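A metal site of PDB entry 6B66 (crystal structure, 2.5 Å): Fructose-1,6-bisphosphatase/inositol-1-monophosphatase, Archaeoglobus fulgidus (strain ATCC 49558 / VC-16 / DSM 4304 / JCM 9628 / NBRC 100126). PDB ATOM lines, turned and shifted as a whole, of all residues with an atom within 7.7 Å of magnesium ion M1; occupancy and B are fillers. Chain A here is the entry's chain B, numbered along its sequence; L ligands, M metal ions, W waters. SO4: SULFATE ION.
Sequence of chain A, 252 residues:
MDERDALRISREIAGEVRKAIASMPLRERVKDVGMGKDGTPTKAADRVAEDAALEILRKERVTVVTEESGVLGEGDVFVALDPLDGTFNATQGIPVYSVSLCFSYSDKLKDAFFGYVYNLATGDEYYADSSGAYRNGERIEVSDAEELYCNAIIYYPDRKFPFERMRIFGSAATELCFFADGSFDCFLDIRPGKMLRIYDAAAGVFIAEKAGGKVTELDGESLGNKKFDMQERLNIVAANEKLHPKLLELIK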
ATOM      1  N   ASP A  38      10.285  -1.417   7.567  1.00  0.00           N
ATOM      2  CA  ASP A  38      10.669  -0.984   8.920  1.00  0.00           C
ATOM      3  C   ASP A  38       9.535  -0.246   9.629  1.00  0.00           C
ATOM      4  O   ASP A  38       9.563  -0.083  10.839  1.00  0.00           O
ATOM      5  CB  ASP A  38      11.897  -0.073   8.877  1.00  0.00           C
ATOM      6  CG  ASP A  38      11.633   1.258   8.138  1.00  0.00           C
ATOM      7  OD1 ASP A  38      11.143   1.250   6.984  1.00  0.00           O
ATOM      8  OD2 ASP A  38      11.941   2.333   8.697  1.00  0.00           O
ATOM      9  N   THR A  40       8.720   2.993   8.553  1.00  0.00           N
ATOM     10  CA  THR A  40       8.893   4.418   8.280  1.00  0.00           C
ATOM     11  C   THR A  40       8.856   4.630   6.782  1.00  0.00           C
ATOM     12  O   THR A  40       9.097   3.691   6.017  1.00  0.00           O
ATOM     13  CB  THR A  40      10.211   5.017   8.847  1.00  0.00           C
ATOM     14  OG1 THR A  40      11.344   4.512   8.109  1.00  0.00           O
ATOM     15  CG2 THR A  40      10.340   4.731  10.343  1.00  0.00           C
ATOM     16  N   PRO A  41       8.506   5.854   6.347  1.00  0.00           N
ATOM     17  CA  PRO A  41       8.371   6.030   4.893  1.00  0.00           C
ATOM     18  C   PRO A  41       9.667   5.790   4.117  1.00  0.00           C
ATOM     19  O   PRO A  41      10.769   5.922   4.671  1.00  0.00           O
ATOM     20  CB  PRO A  41       7.874   7.483   4.745  1.00  0.00           C
ATOM     21  CG  PRO A  41       7.882   8.080   6.115  1.00  0.00           C
ATOM     22  CD  PRO A  41       7.978   6.983   7.115  1.00  0.00           C
ATOM     23  N   ASP A  46      16.036   6.718  -0.648  1.00  0.00           N
ATOM     24  CA  ASP A  46      16.170   5.394  -0.020  1.00  0.00           C
ATOM     25  C   ASP A  46      16.001   4.288  -1.063  1.00  0.00           C
ATOM     26  O   ASP A  46      16.804   3.347  -1.128  1.00  0.00           O
ATOM     27  CB  ASP A  46      15.129   5.190   1.095  1.00  0.00           C
ATOM     28  CG  ASP A  46      15.356   6.101   2.289  1.00  0.00           C
ATOM     29  OD1 ASP A  46      16.485   6.071   2.853  1.00  0.00           O
ATOM     30  OD2 ASP A  46      14.411   6.837   2.668  1.00  0.00           O
ATOM     31  N   THR A  66      17.341  -5.462   5.429  1.00  0.00           N
ATOM     32  CA  THR A  66      17.464  -4.083   4.991  1.00  0.00           C
ATOM     33  C   THR A  66      16.221  -3.241   5.286  1.00  0.00           C
ATOM     34  O   THR A  66      15.099  -3.756   5.313  1.00  0.00           O
ATOM     35  CB  THR A  66      17.813  -4.006   3.502  1.00  0.00           C
ATOM     36  OG1 THR A  66      17.844  -2.638   3.070  1.00  0.00           O
ATOM     37  CG2 THR A  66      16.789  -4.797   2.671  1.00  0.00           C
ATOM     38  N   GLU A  67      16.415  -1.950   5.479  1.00  0.00           N
ATOM     39  CA  GLU A  67      15.388  -1.067   6.008  1.00  0.00           C
ATOM     40  C   GLU A  67      14.115  -1.004   5.200  1.00  0.00           C
ATOM     41  O   GLU A  67      13.025  -1.170   5.739  1.00  0.00           O
ATOM     42  CB  GLU A  67      15.919   0.348   6.202  1.00  0.00           C
ATOM     43  CG  GLU A  67      14.925   1.275   6.881  1.00  0.00           C
ATOM     44  CD  GLU A  67      15.404   2.710   6.919  1.00  0.00           C
ATOM     45  OE1 GLU A  67      16.638   2.898   6.798  1.00  0.00           O
ATOM     46  OE2 GLU A  67      14.558   3.642   7.058  1.00  0.00           O
ATOM     47  N   GLU A  68      14.233  -0.753   3.888  1.00  0.00           N
ATOM     48  CA  GLU A  68      13.025  -0.545   3.090  1.00  0.00           C
ATOM     49  C   GLU A  68      12.294  -1.853   2.764  1.00  0.00           C
ATOM     50  O   GLU A  68      11.099  -1.973   2.997  1.00  0.00           O
ATOM     51  CB  GLU A  68      13.292   0.295   1.826  1.00  0.00           C
ATOM     52  CG  GLU A  68      14.227   1.504   2.013  1.00  0.00           C
ATOM     53  CD  GLU A  68      13.805   2.457   3.123  1.00  0.00           C
ATOM     54  OE1 GLU A  68      14.716   3.024   3.775  1.00  0.00           O
ATOM     55  OE2 GLU A  68      12.597   2.644   3.361  1.00  0.00           O
ATOM     56  N   LEU A  81      21.783  -4.254   6.207  1.00  0.00           N
ATOM     57  CA  LEU A  81      21.984  -3.174   5.245  1.00  0.00           C
ATOM     58  C   LEU A  81      21.126  -1.939   5.542  1.00  0.00           C
ATOM     59  O   LEU A  81      19.899  -2.011   5.555  1.00  0.00           O
ATOM     60  CB  LEU A  81      21.679  -3.677   3.827  1.00  0.00           C
ATOM     61  CG  LEU A  81      21.449  -2.652   2.708  1.00  0.00           C
ATOM     62  CD1 LEU A  81      22.709  -1.876   2.372  1.00  0.00           C
ATOM     63  CD2 LEU A  81      20.897  -3.351   1.471  1.00  0.00           C
ATOM     64  N   ASP A  82      21.789  -0.814   5.789  1.00  0.00           N
ATOM     65  CA  ASP A  82      21.114   0.463   5.708  1.00  0.00           C
ATOM     66  C   ASP A  82      21.584   1.043   4.390  1.00  0.00           C
ATOM     67  O   ASP A  82      22.738   1.450   4.268  1.00  0.00           O
ATOM     68  CB  ASP A  82      21.493   1.384   6.873  1.00  0.00           C
ATOM     69  CG  ASP A  82      20.473   2.499   7.112  1.00  0.00           C
ATOM     70  OD1 ASP A  82      19.648   2.794   6.201  1.00  0.00           O
ATOM     71  OD2 ASP A  82      20.496   3.084   8.221  1.00  0.00           O
ATOM     72  N   PRO A  83      20.703   1.026   3.375  1.00  0.00           N
ATOM     73  CA  PRO A  83      21.130   1.442   2.038  1.00  0.00           C
ATOM     74  C   PRO A  83      21.382   2.952   2.016  1.00  0.00           C
ATOM     75  O   PRO A  83      22.182   3.464   1.220  1.00  0.00           O
ATOM     76  CB  PRO A  83      19.941   1.056   1.165  1.00  0.00           C
ATOM     77  CG  PRO A  83      18.770   1.130   2.079  1.00  0.00           C
ATOM     78  CD  PRO A  83      19.271   0.719   3.439  1.00  0.00           C
ATOM     79  N   LEU A  84      20.721   3.658   2.919  1.00  0.00           N
ATOM     80  CA  LEU A  84      20.941   5.081   3.071  1.00  0.00           C
ATOM     81  C   LEU A  84      20.688   5.498   4.523  1.00  0.00           C
ATOM     82  O   LEU A  84      19.537   5.606   4.954  1.00  0.00           O
ATOM     83  CB  LEU A  84      20.038   5.881   2.121  1.00  0.00           C
ATOM     84  CG  LEU A  84      20.165   7.412   2.169  1.00  0.00           C
ATOM     85  CD1 LEU A  84      21.622   7.865   1.987  1.00  0.00           C
ATOM     86  CD2 LEU A  84      19.232   8.071   1.125  1.00  0.00           C
ATOM     87  N   ASP A  85      21.762   5.716   5.261  1.00  0.00           N
ATOM     88  CA  ASP A  85      21.657   6.117   6.650  1.00  0.00           C
ATOM     89  C   ASP A  85      21.908   7.609   6.729  1.00  0.00           C
ATOM     90  O   ASP A  85      22.947   8.077   6.261  1.00  0.00           O
ATOM     91  CB  ASP A  85      22.673   5.367   7.494  1.00  0.00           C
ATOM     92  CG  ASP A  85      22.499   5.647   8.967  1.00  0.00           C
ATOM     93  OD1 ASP A  85      21.371   5.448   9.485  1.00  0.00           O
ATOM     94  OD2 ASP A  85      23.476   6.107   9.593  1.00  0.00           O
ATOM     95  N   GLY A  86      20.965   8.340   7.302  1.00  0.00           N
ATOM     96  CA  GLY A  86      21.007   9.793   7.293  1.00  0.00           C
ATOM     97  C   GLY A  86      20.240  10.378   6.110  1.00  0.00           C
ATOM     98  O   GLY A  86      20.642  11.392   5.530  1.00  0.00           O
ATOM     99  N   THR A  87      19.129   9.729   5.770  1.00  0.00           N
ATOM    100  CA  THR A  87      18.329  10.111   4.609  1.00  0.00           C
ATOM    101  C   THR A  87      17.934  11.585   4.624  1.00  0.00           C
ATOM    102  O   THR A  87      17.953  12.259   3.587  1.00  0.00           O
ATOM    103  CB  THR A  87      17.062   9.248   4.469  1.00  0.00           C
ATOM    104  OG1 THR A  87      17.426   7.868   4.291  1.00  0.00           O
ATOM    105  CG2 THR A  87      16.228   9.704   3.270  1.00  0.00           C
ATOM    106  N   SER A  98      25.318   7.879   4.566  1.00  0.00           N
ATOM    107  CA  SER A  98      26.158   6.732   4.280  1.00  0.00           C
ATOM    108  C   SER A  98      25.354   5.507   3.905  1.00  0.00           C
ATOM    109  O   SER A  98      24.170   5.415   4.206  1.00  0.00           O
ATOM    110  CB  SER A  98      26.983   6.378   5.506  1.00  0.00           C
ATOM    111  OG  SER A  98      27.867   7.432   5.827  1.00  0.00           O
ATOM    112  N   ARG A 197      17.684   0.635  14.819  1.00  0.00           N
ATOM    113  CA  ARG A 197      17.466  -0.677  14.231  1.00  0.00           C
ATOM    114  C   ARG A 197      18.819  -1.375  14.037  1.00  0.00           C
ATOM    115  O   ARG A 197      19.870  -0.717  14.070  1.00  0.00           O
ATOM    116  CB  ARG A 197      16.754  -0.544  12.877  1.00  0.00           C
ATOM    117  CG  ARG A 197      15.272  -0.143  12.933  1.00  0.00           C
ATOM    118  CD  ARG A 197      15.031   1.356  13.194  1.00  0.00           C
ATOM    119  NE  ARG A 197      15.791   2.256  12.334  1.00  0.00           N
ATOM    120  CZ  ARG A 197      15.483   2.566  11.077  1.00  0.00           C
ATOM    121  NH1 ARG A 197      14.420   2.010  10.495  1.00  0.00           N
ATOM    122  NH2 ARG A 197      16.245   3.411  10.396  1.00  0.00           N
ATOM    123  N   TYR A 199      20.311  -2.467  11.436  1.00  0.00           N
ATOM    124  CA  TYR A 199      21.071  -2.020  10.263  1.00  0.00           C
ATOM    125  C   TYR A 199      21.660  -0.625  10.447  1.00  0.00           C
ATOM    126  O   TYR A 199      22.593  -0.235   9.738  1.00  0.00           O
ATOM    127  CB  TYR A 199      20.249  -2.119   8.965  1.00  0.00           C
ATOM    128  CG  TYR A 199      18.817  -1.738   9.160  1.00  0.00           C
ATOM    129  CD1 TYR A 199      17.839  -2.723   9.242  1.00  0.00           C
ATOM    130  CD2 TYR A 199      18.424  -0.407   9.287  1.00  0.00           C
ATOM    131  CE1 TYR A 199      16.505  -2.387   9.444  1.00  0.00           C
ATOM    132  CE2 TYR A 199      17.104  -0.070   9.486  1.00  0.00           C
ATOM    133  CZ  TYR A 199      16.148  -1.074   9.559  1.00  0.00           C
ATOM    134  OH  TYR A 199      14.838  -0.765   9.763  1.00  0.00           O
ATOM    135  N   ASP A 200      21.130   0.130  11.411  1.00  0.00           N
ATOM    136  CA  ASP A 200      21.716   1.416  11.766  1.00  0.00           C
ATOM    137  C   ASP A 200      23.066   1.268  12.458  1.00  0.00           C
ATOM    138  O   ASP A 200      23.997   2.030  12.207  1.00  0.00           O
ATOM    139  CB  ASP A 200      20.785   2.213  12.680  1.00  0.00           C
ATOM    140  CG  ASP A 200      19.513   2.661  11.977  1.00  0.00           C
ATOM    141  OD1 ASP A 200      19.612   3.282  10.886  1.00  0.00           O
ATOM    142  OD2 ASP A 200      18.425   2.393  12.526  1.00  0.00           O
HETATM  143  S   SO4 L   1      17.719   6.426   8.343  1.00  0.00           S
HETATM  144  O1  SO4 L   1      17.994   6.242   9.777  1.00  0.00           O
HETATM  145  O2  SO4 L   1      18.320   5.260   7.680  1.00  0.00           O
HETATM  146  O3  SO4 L   1      16.269   6.496   8.115  1.00  0.00           O
HETATM  147  O4  SO4 L   1      18.311   7.695   7.868  1.00  0.00           O
HETATM  148 MG    MG M   1      18.065   4.168   5.935  1.00  0.00          MG
HETATM  149 MG    MG M   2      12.006   3.495   6.056  1.00  0.00          MG
HETATM  150  O   HOH W   1      17.470   3.838   3.976  1.00  0.00           O
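Water W1 lies within hydrogen-bond range of OD1 of Asp 46 (2.7 Å), OE1 of Glu 68 (2.9 Å) and N of Leu 84 (3.4 Å).
Magnesium ion M1 is bound by water W1 (2.1 Å), O2 of the ligand (2.1 Å), OE1 of Glu 67 (2.1 Å), OD1 of Asp 82 (2.1 Å) and O of Leu 84 (2.3 Å).
Magnesium ion M1 has five donor atoms within binding distance.
The side-chain carboxylate (OD1) of Asp 46 lies within hydrogen-bond range of the side-chain hydroxyl (OG1) of Thr 87.
The backbone carbonyl oxygen (O) of Leu 81 lies within hydrogen-bond range of the backbone NH (N) of Glu 67 (3.5 Å).
OE2 of Glu 67 is in salt-bridge range of NH2 of Arg 197 (3.7 Å).
The side-chain hydroxyl of Thr 40 lies close to the side-chain carboxylate of Glu 67, 3.5 Å away.
O of Leu 84 lies close to OG1 of Thr 87, at 3.2 Å.
O of Glu 67 sits at hydrogen-bond distance from N of Asp 38 (3.3 Å).
Merely in contact with magnesium ion M1: Asp 46 (3.95 Å).
Within 4 Å of magnesium ion M1: Asp 46, Glu 67, Asp 82 and Leu 84.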
